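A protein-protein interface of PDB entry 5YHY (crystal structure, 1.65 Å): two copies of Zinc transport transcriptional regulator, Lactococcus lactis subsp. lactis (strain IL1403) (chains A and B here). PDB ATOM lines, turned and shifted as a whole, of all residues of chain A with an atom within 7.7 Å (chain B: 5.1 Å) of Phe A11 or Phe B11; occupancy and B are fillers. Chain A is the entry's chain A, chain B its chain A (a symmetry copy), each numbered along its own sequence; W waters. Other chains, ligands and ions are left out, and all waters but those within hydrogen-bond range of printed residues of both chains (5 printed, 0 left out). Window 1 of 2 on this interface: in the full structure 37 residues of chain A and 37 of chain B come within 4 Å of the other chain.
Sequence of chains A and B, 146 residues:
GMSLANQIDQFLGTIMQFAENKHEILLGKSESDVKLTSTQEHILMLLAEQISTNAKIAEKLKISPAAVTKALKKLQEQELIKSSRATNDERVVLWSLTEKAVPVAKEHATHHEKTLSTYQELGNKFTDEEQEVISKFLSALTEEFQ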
ATOM      1  N   MET A   2      -5.916 -23.144 -21.091  1.00  0.00           N
ATOM      2  CA  MET A   2      -4.559 -23.095 -21.633  1.00  0.00           C
ATOM      3  C   MET A   2      -3.887 -24.460 -21.495  1.00  0.00           C
ATOM      4  O   MET A   2      -4.118 -25.159 -20.509  1.00  0.00           O
ATOM      5  CB  MET A   2      -3.762 -22.034 -20.868  1.00  0.00           C
ATOM      6  CG  MET A   2      -2.330 -21.857 -21.315  1.00  0.00           C
ATOM      7  SD  MET A   2      -1.439 -20.630 -20.329  1.00  0.00           S
ATOM      8  CE  MET A   2      -2.435 -19.164 -20.608  1.00  0.00           C
ATOM      9  N   LEU A   4      -0.999 -27.211 -20.720  1.00  0.00           N
ATOM     10  CA  LEU A   4      -0.014 -27.236 -19.646  1.00  0.00           C
ATOM     11  C   LEU A   4       1.318 -26.701 -20.155  1.00  0.00           C
ATOM     12  O   LEU A   4       2.018 -25.997 -19.432  1.00  0.00           O
ATOM     13  CB  LEU A   4       0.162 -28.638 -19.062  1.00  0.00           C
ATOM     14  CG  LEU A   4       1.094 -28.735 -17.847  1.00  0.00           C
ATOM     15  CD1 LEU A   4       0.535 -27.980 -16.638  1.00  0.00           C
ATOM     16  CD2 LEU A   4       1.380 -30.185 -17.479  1.00  0.00           C
ATOM     17  N   ALA A   5       1.673 -27.038 -21.391  1.00  0.00           N
ATOM     18  CA  ALA A   5       2.915 -26.528 -21.969  1.00  0.00           C
ATOM     19  C   ALA A   5       2.960 -25.007 -21.922  1.00  0.00           C
ATOM     20  O   ALA A   5       3.972 -24.415 -21.549  1.00  0.00           O
ATOM     21  CB  ALA A   5       3.090 -27.016 -23.410  1.00  0.00           C
ATOM     22  N   ASN A   6       1.862 -24.371 -22.314  1.00  0.00           N
ATOM     23  CA  ASN A   6       1.798 -22.925 -22.294  1.00  0.00           C
ATOM     24  C   ASN A   6       1.823 -22.380 -20.868  1.00  0.00           C
ATOM     25  O   ASN A   6       2.467 -21.371 -20.602  1.00  0.00           O
ATOM     26  CB  ASN A   6       0.570 -22.442 -23.059  1.00  0.00           C
ATOM     27  CG  ASN A   6       0.783 -22.491 -24.554  1.00  0.00           C
ATOM     28  OD1 ASN A   6       1.849 -22.116 -25.045  1.00  0.00           O
ATOM     29  ND2 ASN A   6      -0.214 -22.970 -25.286  1.00  0.00           N
ATOM     30  N   GLN A   7       1.174 -23.086 -19.952  1.00  0.00           N
ATOM     31  CA  GLN A   7       1.199 -22.685 -18.543  1.00  0.00           C
ATOM     32  C   GLN A   7       2.623 -22.733 -18.003  1.00  0.00           C
ATOM     33  O   GLN A   7       3.048 -21.856 -17.232  1.00  0.00           O
ATOM     34  CB  GLN A   7       0.341 -23.620 -17.694  1.00  0.00           C
ATOM     35  CG  GLN A   7      -1.140 -23.638 -18.005  1.00  0.00           C
ATOM     36  CD  GLN A   7      -1.876 -24.552 -17.059  1.00  0.00           C
ATOM     37  OE1 GLN A   7      -1.519 -24.651 -15.873  1.00  0.00           O
ATOM     38  NE2 GLN A   7      -2.880 -25.268 -17.581  1.00  0.00           N
ATOM     39  N   ILE A   8       3.359 -23.769 -18.387  1.00  0.00           N
ATOM     40  CA  ILE A   8       4.747 -23.888 -17.938  1.00  0.00           C
ATOM     41  C   ILE A   8       5.583 -22.739 -18.487  1.00  0.00           C
ATOM     42  O   ILE A   8       6.360 -22.113 -17.753  1.00  0.00           O
ATOM     43  CB  ILE A   8       5.355 -25.248 -18.334  1.00  0.00           C
ATOM     44  CG1 ILE A   8       4.661 -26.379 -17.557  1.00  0.00           C
ATOM     45  CG2 ILE A   8       6.865 -25.262 -18.076  1.00  0.00           C
ATOM     46  CD1 ILE A   8       4.875 -27.751 -18.180  1.00  0.00           C
ATOM     47  N   ASP A   9       5.412 -22.464 -19.778  1.00  0.00           N
ATOM     48  CA  ASP A   9       6.130 -21.377 -20.447  1.00  0.00           C
ATOM     49  C   ASP A   9       5.888 -20.051 -19.725  1.00  0.00           C
ATOM     50  O   ASP A   9       6.831 -19.307 -19.429  1.00  0.00           O
ATOM     51  CB  ASP A   9       5.646 -21.295 -21.898  1.00  0.00           C
ATOM     52  CG  ASP A   9       6.531 -20.426 -22.774  1.00  0.00           C
ATOM     53  OD1 ASP A   9       7.766 -20.423 -22.588  1.00  0.00           O
ATOM     54  OD2 ASP A   9       5.979 -19.754 -23.674  1.00  0.00           O
ATOM     55  N   GLN A  10       4.629 -19.776 -19.408  1.00  0.00           N
ATOM     56  CA  GLN A  10       4.271 -18.529 -18.742  1.00  0.00           C
ATOM     57  C   GLN A  10       4.797 -18.457 -17.311  1.00  0.00           C
ATOM     58  O   GLN A  10       5.239 -17.404 -16.863  1.00  0.00           O
ATOM     59  CB  GLN A  10       2.765 -18.292 -18.800  1.00  0.00           C
ATOM     60  CG  GLN A  10       2.288 -18.051 -20.224  1.00  0.00           C
ATOM     61  CD  GLN A  10       0.831 -17.650 -20.307  1.00  0.00           C
ATOM     62  OE1 GLN A  10       0.196 -17.331 -19.295  1.00  0.00           O
ATOM     63  NE2 GLN A  10       0.291 -17.656 -21.524  1.00  0.00           N
ATOM     64  N   PHE A  11       4.756 -19.587 -16.608  1.00  0.00           N
ATOM     65  CA  PHE A  11       5.290 -19.661 -15.262  1.00  0.00           C
ATOM     66  C   PHE A  11       6.778 -19.327 -15.246  1.00  0.00           C
ATOM     67  O   PHE A  11       7.254 -18.597 -14.387  1.00  0.00           O
ATOM     68  CB  PHE A  11       5.061 -21.060 -14.677  1.00  0.00           C
ATOM     69  CG  PHE A  11       5.802 -21.299 -13.397  1.00  0.00           C
ATOM     70  CD1 PHE A  11       5.355 -20.741 -12.218  1.00  0.00           C
ATOM     71  CD2 PHE A  11       6.938 -22.084 -13.378  1.00  0.00           C
ATOM     72  CE1 PHE A  11       6.032 -20.961 -11.034  1.00  0.00           C
ATOM     73  CE2 PHE A  11       7.615 -22.306 -12.199  1.00  0.00           C
ATOM     74  CZ  PHE A  11       7.160 -21.740 -11.030  1.00  0.00           C
ATOM     75  N   LEU A  12       7.521 -19.877 -16.195  1.00  0.00           N
ATOM     76  CA  LEU A  12       8.954 -19.657 -16.230  1.00  0.00           C
ATOM     77  C   LEU A  12       9.248 -18.208 -16.581  1.00  0.00           C
ATOM     78  O   LEU A  12      10.212 -17.632 -16.079  1.00  0.00           O
ATOM     79  CB  LEU A  12       9.627 -20.623 -17.197  1.00  0.00           C
ATOM     80  CG  LEU A  12       9.552 -22.051 -16.670  1.00  0.00           C
ATOM     81  CD1 LEU A  12      10.014 -23.042 -17.727  1.00  0.00           C
ATOM     82  CD2 LEU A  12      10.379 -22.180 -15.386  1.00  0.00           C
ATOM     83  N   GLY A  13       8.392 -17.620 -17.411  1.00  0.00           N
ATOM     84  CA  GLY A  13       8.468 -16.189 -17.686  1.00  0.00           C
ATOM     85  C   GLY A  13       8.313 -15.351 -16.423  1.00  0.00           C
ATOM     86  O   GLY A  13       9.089 -14.420 -16.180  1.00  0.00           O
ATOM     87  N   THR A  14       7.316 -15.686 -15.609  1.00  0.00           N
ATOM     88  CA  THR A  14       7.104 -15.007 -14.335  1.00  0.00           C
ATOM     89  C   THR A  14       8.351 -15.081 -13.460  1.00  0.00           C
ATOM     90  O   THR A  14       8.765 -14.084 -12.860  1.00  0.00           O
ATOM     91  CB  THR A  14       5.912 -15.619 -13.584  1.00  0.00           C
ATOM     92  OG1 THR A  14       4.726 -15.452 -14.370  1.00  0.00           O
ATOM     93  CG2 THR A  14       5.724 -14.944 -12.235  1.00  0.00           C
ATOM     94  N   ILE A  15       8.956 -16.264 -13.390  1.00  0.00           N
ATOM     95  CA  ILE A  15      10.144 -16.452 -12.565  1.00  0.00           C
ATOM     96  C   ILE A  15      11.332 -15.657 -13.098  1.00  0.00           C
ATOM     97  O   ILE A  15      12.052 -15.015 -12.329  1.00  0.00           O
ATOM     98  CB  ILE A  15      10.531 -17.934 -12.433  1.00  0.00           C
ATOM     99  CG1 ILE A  15       9.384 -18.724 -11.798  1.00  0.00           C
ATOM    100  CG2 ILE A  15      11.816 -18.072 -11.612  1.00  0.00           C
ATOM    101  CD1 ILE A  15       8.841 -18.092 -10.526  1.00  0.00           C
ATOM    102  N   MET A  16      11.543 -15.701 -14.408  1.00  0.00           N
ATOM    103  CA  MET A  16      12.607 -14.910 -15.016  1.00  0.00           C
ATOM    104  C   MET A  16      12.483 -13.440 -14.631  1.00  0.00           C
ATOM    105  O   MET A  16      13.467 -12.816 -14.226  1.00  0.00           O
ATOM    106  CB  MET A  16      12.598 -15.050 -16.541  1.00  0.00           C
ATOM    107  CG  MET A  16      13.437 -13.983 -17.232  1.00  0.00           C
ATOM    108  SD  MET A  16      13.587 -14.243 -19.010  1.00  0.00           S
ATOM    109  CE  MET A  16      14.986 -15.362 -19.061  1.00  0.00           C
ATOM    110  N   GLN A  17      11.279 -12.892 -14.754  1.00  0.00           N
ATOM    111  CA  GLN A  17      11.041 -11.485 -14.419  1.00  0.00           C
ATOM    112  C   GLN A  17      11.374 -11.173 -12.968  1.00  0.00           C
ATOM    113  O   GLN A  17      11.982 -10.143 -12.656  1.00  0.00           O
ATOM    114  CB  GLN A  17       9.585 -11.110 -14.688  1.00  0.00           C
ATOM    115  CG  GLN A  17       9.196 -11.197 -16.151  1.00  0.00           C
ATOM    116  CD  GLN A  17       7.747 -10.815 -16.382  1.00  0.00           C
ATOM    117  OE1 GLN A  17       7.140 -10.113 -15.568  1.00  0.00           O
ATOM    118  NE2 GLN A  17       7.182 -11.283 -17.491  1.00  0.00           N
ATOM    119  N   ILE A  25      16.481 -16.193  -5.241  1.00  0.00           N
ATOM    120  CA  ILE A  25      15.032 -16.049  -5.219  1.00  0.00           C
ATOM    121  C   ILE A  25      14.552 -16.059  -3.766  1.00  0.00           C
ATOM    122  O   ILE A  25      14.542 -17.097  -3.109  1.00  0.00           O
ATOM    123  CB  ILE A  25      14.337 -17.173  -6.010  1.00  0.00           C
ATOM    124  CG1 ILE A  25      14.759 -17.136  -7.483  1.00  0.00           C
ATOM    125  CG2 ILE A  25      12.815 -17.052  -5.890  1.00  0.00           C
ATOM    126  CD1 ILE A  25      14.310 -15.903  -8.206  1.00  0.00           C
ATOM    127  N   PHE A 137       7.347 -33.985 -11.457  1.00  0.00           N
ATOM    128  CA  PHE A 137       7.306 -32.904 -12.430  1.00  0.00           C
ATOM    129  C   PHE A 137       8.519 -31.969 -12.290  1.00  0.00           C
ATOM    130  O   PHE A 137       9.207 -31.663 -13.274  1.00  0.00           O
ATOM    131  CB  PHE A 137       6.001 -32.103 -12.284  1.00  0.00           C
ATOM    132  CG  PHE A 137       5.967 -30.878 -13.144  1.00  0.00           C
ATOM    133  CD1 PHE A 137       5.752 -30.991 -14.511  1.00  0.00           C
ATOM    134  CD2 PHE A 137       6.160 -29.625 -12.591  1.00  0.00           C
ATOM    135  CE1 PHE A 137       5.740 -29.874 -15.310  1.00  0.00           C
ATOM    136  CE2 PHE A 137       6.148 -28.495 -13.397  1.00  0.00           C
ATOM    137  CZ  PHE A 137       5.939 -28.631 -14.753  1.00  0.00           C
ATOM    138  N   LEU A 138       8.775 -31.503 -11.075  1.00  0.00           N
ATOM    139  CA  LEU A 138       9.877 -30.575 -10.862  1.00  0.00           C
ATOM    140  C   LEU A 138      11.216 -31.204 -11.199  1.00  0.00           C
ATOM    141  O   LEU A 138      12.088 -30.546 -11.762  1.00  0.00           O
ATOM    142  CB  LEU A 138       9.895 -30.053  -9.430  1.00  0.00           C
ATOM    143  CG  LEU A 138       8.710 -29.161  -9.073  1.00  0.00           C
ATOM    144  CD1 LEU A 138       8.841 -28.779  -7.607  1.00  0.00           C
ATOM    145  CD2 LEU A 138       8.678 -27.932  -9.969  1.00  0.00           C
ATOM    146  N   SER A 139      11.390 -32.469 -10.817  1.00  0.00           N
ATOM    147  CA  SER A 139      12.638 -33.174 -11.092  1.00  0.00           C
ATOM    148  C   SER A 139      12.884 -33.271 -12.589  1.00  0.00           C
ATOM    149  O   SER A 139      13.988 -33.007 -13.062  1.00  0.00           O
ATOM    150  CB  SER A 139      12.603 -34.564 -10.462  1.00  0.00           C
ATOM    151  OG  SER A 139      12.667 -34.458  -9.054  1.00  0.00           O
ATOM    152  N   ALA A 140      11.839 -33.621 -13.331  1.00  0.00           N
ATOM    153  CA  ALA A 140      11.954 -33.784 -14.774  1.00  0.00           C
ATOM    154  C   ALA A 140      12.207 -32.452 -15.455  1.00  0.00           C
ATOM    155  O   ALA A 140      13.033 -32.353 -16.369  1.00  0.00           O
ATOM    156  CB  ALA A 140      10.702 -34.434 -15.338  1.00  0.00           C
ATOM    157  N   LEU A 141      11.498 -31.416 -15.015  1.00  0.00           N
ATOM    158  CA  LEU A 141      11.667 -30.105 -15.625  1.00  0.00           C
ATOM    159  C   LEU A 141      13.071 -29.569 -15.350  1.00  0.00           C
ATOM    160  O   LEU A 141      13.700 -28.961 -16.214  1.00  0.00           O
ATOM    161  CB  LEU A 141      10.607 -29.149 -15.094  1.00  0.00           C
ATOM    162  CG  LEU A 141      10.527 -27.782 -15.758  1.00  0.00           C
ATOM    163  CD1 LEU A 141      10.401 -27.922 -17.271  1.00  0.00           C
ATOM    164  CD2 LEU A 141       9.347 -27.011 -15.184  1.00  0.00           C
ATOM    165  N   THR A 142      13.560 -29.815 -14.141  1.00  0.00           N
ATOM    166  CA  THR A 142      14.911 -29.387 -13.769  1.00  0.00           C
ATOM    167  C   THR A 142      15.953 -29.930 -14.740  1.00  0.00           C
ATOM    168  O   THR A 142      16.902 -29.229 -15.089  1.00  0.00           O
ATOM    169  CB  THR A 142      15.270 -29.865 -12.357  1.00  0.00           C
ATOM    170  OG1 THR A 142      14.486 -29.140 -11.407  1.00  0.00           O
ATOM    171  CG2 THR A 142      16.749 -29.640 -12.067  1.00  0.00           C
ATOM    172  N   GLU A 143      15.763 -31.168 -15.183  1.00  0.00           N
ATOM    173  CA  GLU A 143      16.726 -31.812 -16.075  1.00  0.00           C
ATOM    174  C   GLU A 143      16.858 -31.084 -17.411  1.00  0.00           C
ATOM    175  O   GLU A 143      17.887 -31.179 -18.077  1.00  0.00           O
ATOM    176  CB  GLU A 143      16.345 -33.267 -16.324  1.00  0.00           C
ATOM    177  CG  GLU A 143      16.371 -34.138 -15.073  1.00  0.00           C
ATOM    178  CD  GLU A 143      16.197 -35.610 -15.397  1.00  0.00           C
ATOM    179  OE1 GLU A 143      16.171 -35.963 -16.598  1.00  0.00           O
ATOM    180  OE2 GLU A 143      16.100 -36.418 -14.452  1.00  0.00           O
ATOM    181  N   PHE A 145      16.987 -27.953 -17.858  1.00  0.00           N
ATOM    182  CA  PHE A 145      17.699 -26.694 -17.708  1.00  0.00           C
ATOM    183  C   PHE A 145      19.141 -26.855 -17.255  1.00  0.00           C
ATOM    184  O   PHE A 145      19.781 -25.889 -16.838  1.00  0.00           O
ATOM    185  CB  PHE A 145      16.911 -25.753 -16.791  1.00  0.00           C
ATOM    186  CG  PHE A 145      15.606 -25.323 -17.387  1.00  0.00           C
ATOM    187  CD1 PHE A 145      15.569 -24.309 -18.330  1.00  0.00           C
ATOM    188  CD2 PHE A 145      14.425 -25.960 -17.061  1.00  0.00           C
ATOM    189  CE1 PHE A 145      14.380 -23.922 -18.909  1.00  0.00           C
ATOM    190  CE2 PHE A 145      13.235 -25.573 -17.636  1.00  0.00           C
ATOM    191  CZ  PHE A 145      13.213 -24.557 -18.567  1.00  0.00           C
ATOM    192  N   ASN B   6      11.942 -27.517   0.053  1.00  0.00           N
ATOM    193  CA  ASN B   6      13.330 -27.423  -0.347  1.00  0.00           C
ATOM    194  C   ASN B   6      13.510 -27.729  -1.832  1.00  0.00           C
ATOM    195  O   ASN B   6      14.296 -27.075  -2.508  1.00  0.00           O
ATOM    196  CB  ASN B   6      14.191 -28.332   0.523  1.00  0.00           C
ATOM    197  CG  ASN B   6      14.459 -27.724   1.880  1.00  0.00           C
ATOM    198  OD1 ASN B   6      14.741 -26.530   1.984  1.00  0.00           O
ATOM    199  ND2 ASN B   6      14.352 -28.530   2.929  1.00  0.00           N
ATOM    200  N   GLN B   7      12.735 -28.679  -2.340  1.00  0.00           N
ATOM    201  CA  GLN B   7      12.782 -28.997  -3.770  1.00  0.00           C
ATOM    202  C   GLN B   7      12.355 -27.790  -4.595  1.00  0.00           C
ATOM    203  O   GLN B   7      12.934 -27.498  -5.655  1.00  0.00           O
ATOM    204  CB  GLN B   7      11.843 -30.153  -4.103  1.00  0.00           C
ATOM    205  CG  GLN B   7      12.164 -31.485  -3.459  1.00  0.00           C
ATOM    206  CD  GLN B   7      11.199 -32.549  -3.916  1.00  0.00           C
ATOM    207  OE1 GLN B   7      10.761 -32.544  -5.079  1.00  0.00           O
ATOM    208  NE2 GLN B   7      10.818 -33.444  -2.997  1.00  0.00           N
ATOM    209  N   ILE B   8      11.324 -27.097  -4.126  1.00  0.00           N
ATOM    210  CA  ILE B   8      10.856 -25.908  -4.840  1.00  0.00           C
ATOM    211  C   ILE B   8      11.933 -24.831  -4.839  1.00  0.00           C
ATOM    212  O   ILE B   8      12.219 -24.220  -5.879  1.00  0.00           O
ATOM    213  CB  ILE B   8       9.541 -25.369  -4.240  1.00  0.00           C
ATOM    214  CG1 ILE B   8       8.402 -26.371  -4.491  1.00  0.00           C
ATOM    215  CG2 ILE B   8       9.197 -24.000  -4.833  1.00  0.00           C
ATOM    216  CD1 ILE B   8       7.200 -26.148  -3.585  1.00  0.00           C
ATOM    217  N   ASP B   9      12.530 -24.609  -3.671  1.00  0.00           N
ATOM    218  CA  ASP B   9      13.599 -23.619  -3.514  1.00  0.00           C
ATOM    219  C   ASP B   9      14.738 -23.901  -4.494  1.00  0.00           C
ATOM    220  O   ASP B   9      15.210 -22.998  -5.197  1.00  0.00           O
ATOM    221  CB  ASP B   9      14.105 -23.675  -2.070  1.00  0.00           C
ATOM    222  CG  ASP B   9      14.983 -22.492  -1.700  1.00  0.00           C
ATOM    223  OD1 ASP B   9      14.721 -21.364  -2.165  1.00  0.00           O
ATOM    224  OD2 ASP B   9      15.936 -22.698  -0.915  1.00  0.00           O
ATOM    225  N   GLN B  10      15.151 -25.160  -4.568  1.00  0.00           N
ATOM    226  CA  GLN B  10      16.250 -25.545  -5.447  1.00  0.00           C
ATOM    227  C   GLN B  10      15.887 -25.427  -6.925  1.00  0.00           C
ATOM    228  O   GLN B  10      16.708 -25.011  -7.735  1.00  0.00           O
ATOM    229  CB  GLN B  10      16.759 -26.941  -5.103  1.00  0.00           C
ATOM    230  CG  GLN B  10      17.410 -26.980  -3.729  1.00  0.00           C
ATOM    231  CD  GLN B  10      18.074 -28.305  -3.418  1.00  0.00           C
ATOM    232  OE1 GLN B  10      18.253 -29.153  -4.299  1.00  0.00           O
ATOM    233  NE2 GLN B  10      18.450 -28.487  -2.154  1.00  0.00           N
ATOM    234  N   PHE B  11      14.649 -25.785  -7.260  1.00  0.00           N
ATOM    235  CA  PHE B  11      14.165 -25.652  -8.621  1.00  0.00           C
ATOM    236  C   PHE B  11      14.215 -24.198  -9.079  1.00  0.00           C
ATOM    237  O   PHE B  11      14.625 -23.898 -10.192  1.00  0.00           O
ATOM    238  CB  PHE B  11      12.733 -26.187  -8.729  1.00  0.00           C
ATOM    239  CG  PHE B  11      12.070 -25.857 -10.032  1.00  0.00           C
ATOM    240  CD1 PHE B  11      12.405 -26.545 -11.179  1.00  0.00           C
ATOM    241  CD2 PHE B  11      11.113 -24.863 -10.102  1.00  0.00           C
ATOM    242  CE1 PHE B  11      11.794 -26.247 -12.381  1.00  0.00           C
ATOM    243  CE2 PHE B  11      10.501 -24.565 -11.299  1.00  0.00           C
ATOM    244  CZ  PHE B  11      10.848 -25.258 -12.438  1.00  0.00           C
ATOM    245  N   LEU B  12      13.781 -23.289  -8.218  1.00  0.00           N
ATOM    246  CA  LEU B  12      13.742 -21.887  -8.583  1.00  0.00           C
ATOM    247  C   LEU B  12      15.157 -21.348  -8.723  1.00  0.00           C
ATOM    248  O   LEU B  12      15.416 -20.501  -9.576  1.00  0.00           O
ATOM    249  CB  LEU B  12      12.927 -21.086  -7.576  1.00  0.00           C
ATOM    250  CG  LEU B  12      11.452 -21.461  -7.658  1.00  0.00           C
ATOM    251  CD1 LEU B  12      10.672 -20.840  -6.509  1.00  0.00           C
ATOM    252  CD2 LEU B  12      10.878 -21.038  -9.015  1.00  0.00           C
ATOM    253  N   GLY B  13      16.067 -21.872  -7.908  1.00  0.00           N
ATOM    254  CA  GLY B  13      17.485 -21.566  -8.063  1.00  0.00           C
ATOM    255  C   GLY B  13      18.016 -21.967  -9.433  1.00  0.00           C
ATOM    256  O   GLY B  13      18.709 -21.188 -10.097  1.00  0.00           O
ATOM    257  N   THR B  14      17.682 -23.179  -9.865  1.00  0.00           N
ATOM    258  CA  THR B  14      18.068 -23.656 -11.189  1.00  0.00           C
ATOM    259  C   THR B  14      17.569 -22.712 -12.278  1.00  0.00           C
ATOM    260  O   THR B  14      18.305 -22.371 -13.209  1.00  0.00           O
ATOM    261  CB  THR B  14      17.520 -25.068 -11.441  1.00  0.00           C
ATOM    262  OG1 THR B  14      18.077 -25.967 -10.474  1.00  0.00           O
ATOM    263  CG2 THR B  14      17.880 -25.543 -12.839  1.00  0.00           C
ATOM    264  N   ILE B  15      16.314 -22.286 -12.161  1.00  0.00           N
ATOM    265  CA  ILE B  15      15.727 -21.398 -13.160  1.00  0.00           C
ATOM    266  C   ILE B  15      16.399 -20.028 -13.161  1.00  0.00           C
ATOM    267  O   ILE B  15      16.702 -19.480 -14.223  1.00  0.00           O
ATOM    268  CB  ILE B  15      14.212 -21.230 -12.968  1.00  0.00           C
ATOM    269  CG1 ILE B  15      13.512 -22.587 -13.072  1.00  0.00           C
ATOM    270  CG2 ILE B  15      13.656 -20.242 -13.999  1.00  0.00           C
ATOM    271  CD1 ILE B  15      13.913 -23.384 -14.304  1.00  0.00           C
ATOM    272  N   LEU B 138       1.244 -24.788 -10.099  1.00  0.00           N
ATOM    273  CA  LEU B 138       1.883 -23.691 -10.812  1.00  0.00           C
ATOM    274  C   LEU B 138       1.121 -22.389 -10.642  1.00  0.00           C
ATOM    275  O   LEU B 138       1.727 -21.329 -10.502  1.00  0.00           O
ATOM    276  CB  LEU B 138       2.041 -24.008 -12.295  1.00  0.00           C
ATOM    277  CG  LEU B 138       3.020 -25.139 -12.593  1.00  0.00           C
ATOM    278  CD1 LEU B 138       3.017 -25.373 -14.095  1.00  0.00           C
ATOM    279  CD2 LEU B 138       4.411 -24.788 -12.087  1.00  0.00           C
ATOM    280  N   LEU B 141       1.768 -21.098  -7.091  1.00  0.00           N
ATOM    281  CA  LEU B 141       3.134 -20.623  -6.922  1.00  0.00           C
ATOM    282  C   LEU B 141       3.330 -19.298  -7.657  1.00  0.00           C
ATOM    283  O   LEU B 141       4.002 -18.392  -7.166  1.00  0.00           O
ATOM    284  CB  LEU B 141       4.112 -21.674  -7.430  1.00  0.00           C
ATOM    285  CG  LEU B 141       5.589 -21.417  -7.167  1.00  0.00           C
ATOM    286  CD1 LEU B 141       5.834 -21.138  -5.688  1.00  0.00           C
ATOM    287  CD2 LEU B 141       6.401 -22.616  -7.635  1.00  0.00           C
ATOM    288  N   THR B 142       2.723 -19.189  -8.832  1.00  0.00           N
ATOM    289  CA  THR B 142       2.802 -17.953  -9.614  1.00  0.00           C
ATOM    290  C   THR B 142       2.326 -16.752  -8.805  1.00  0.00           C
ATOM    291  O   THR B 142       2.908 -15.672  -8.896  1.00  0.00           O
ATOM    292  CB  THR B 142       1.949 -18.050 -10.885  1.00  0.00           C
ATOM    293  OG1 THR B 142       2.557 -18.979 -11.784  1.00  0.00           O
ATOM    294  CG2 THR B 142       1.831 -16.693 -11.565  1.00  0.00           C
HETATM  295  O   HOH W   1      16.201 -19.021  -1.862  1.00  0.00           O
HETATM  296  O   HOH W   2      13.432 -19.644  -3.744  1.00  0.00           O
HETATM  297  O   HOH W   3      20.497 -23.898 -14.478  1.00  0.00           O
HETATM  298  O   HOH W   4       2.755 -17.867 -14.535  1.00  0.00           O
HETATM  299  O   HOH W   5      16.161 -28.073  -9.193  1.00  0.00           O
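The backbone carbonyl oxygen of Leu B138 is in hydrogen-bond range of the side-chain hydroxyl of Thr B142.
The backbone carbonyl oxygen (O) of Leu A138 sits at hydrogen-bond distance from the side-chain hydroxyl (OG1) of Thr A142 (2.8 Å).
Hydrophobic or aromatic side chains of chain A within 4 Å of the printed part of chain B: Ile A8, Phe A11, Leu A12, Ile A15, Leu A138, Leu A141 and Phe A145.
Hydrophobic or aromatic side chains of chain B within 4 Å of the printed part of chain A: Ile B8, Phe B11, Leu B12, Ile B15, Leu B138 and Leu B141.
Among the printed residues, no Asp or Glu carboxylate lies within 4 Å of a Lys or Arg side-chain nitrogen of the other chain.
Of chain B, only Phe B11, Leu B138, Leu B141 and Thr B142 come within 4 Å of Phe A11.
Printed residues of chain A within 4 Å of Phe B11: Phe A11, Leu A138, Leu A141 and Thr A142.
Printed residues of chain A within 4 Å of Ile B8: Leu A138 (3.96 Å).
Of the printed residues of chain A, Leu B138 touches Ile A8 (3.96 Å) and Phe A11 (3.9 Å).
Of the printed residues of chain B, Phe A145 touches Ile B15 (3.8 Å).
Ala A140 touches none of the printed residues of chain B.
The nearest residue of chain B that does not touch Phe A11 is Leu B12 (4.3 Å).
The nearest residue of chain A that does not touch Phe B11 is Leu A12 (4.3 Å).
The nearest printed residue of chain B that does not touch Thr A142 is Thr B14 (4.2 Å).
Phe B11 touches its own counterpart, Phe A11.
Phe A11 touches Leu B141, and with the chains exchanged Leu A141 touches Phe B11.
Phe A11 touches Thr B142, and with the chains exchanged Thr A142 touches Phe B11.
Leu A12 touches Ile B15, and with the chains exchanged Ile A15 touches Leu B12.
13 positions are printed for both chains.
Of the 13 pairs that touch across the chains among the printed residues, 12 have their exchanged pair printed and touching as well.
Water W2 lies within hydrogen-bond range of the side-chain carboxylate (OD1) of Asp B9 (2.7 Å) and the backbone carbonyl oxygen (O) of Ile A25 (2.9 Å).
Water W1 lies within hydrogen-bond range of the side-chain carboxylate (OD1) of Asp B9 (2.8 Å) and the backbone carbonyl oxygen (O) of Ile A25 (2.8 Å).
Water W3 lies within hydrogen-bond range of O of Thr B14 and O of Phe A145.
Water W5 lies within hydrogen-bond range of OG1 of Thr A142, OG1 of Thr B14, N of Phe B11 and O of Gln B10.
Water W4 lies within hydrogen-bond range of OG1 of Thr B142 (3.0 Å), OG1 of Thr A14 (3.1 Å), N of Phe A11 (3.4 Å) and O of Gln A10 (3.4 Å).
Among the printed residues, merely in contact across the chains: Thr A142 with Phe B11, Phe A11 with Thr B142, Leu A141 with Phe B11, Phe A11 with Leu B141, Ile A15 with Ile B15, Phe A11 with Phe B11, Phe A145 with Ile B15, Leu A12 with Ile B15, Ile A15 with Leu B12, Phe A11 with Leu B138, Leu A138 with Phe B11, Ile A8 with Leu B138 and Leu A138 with Ile B8.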
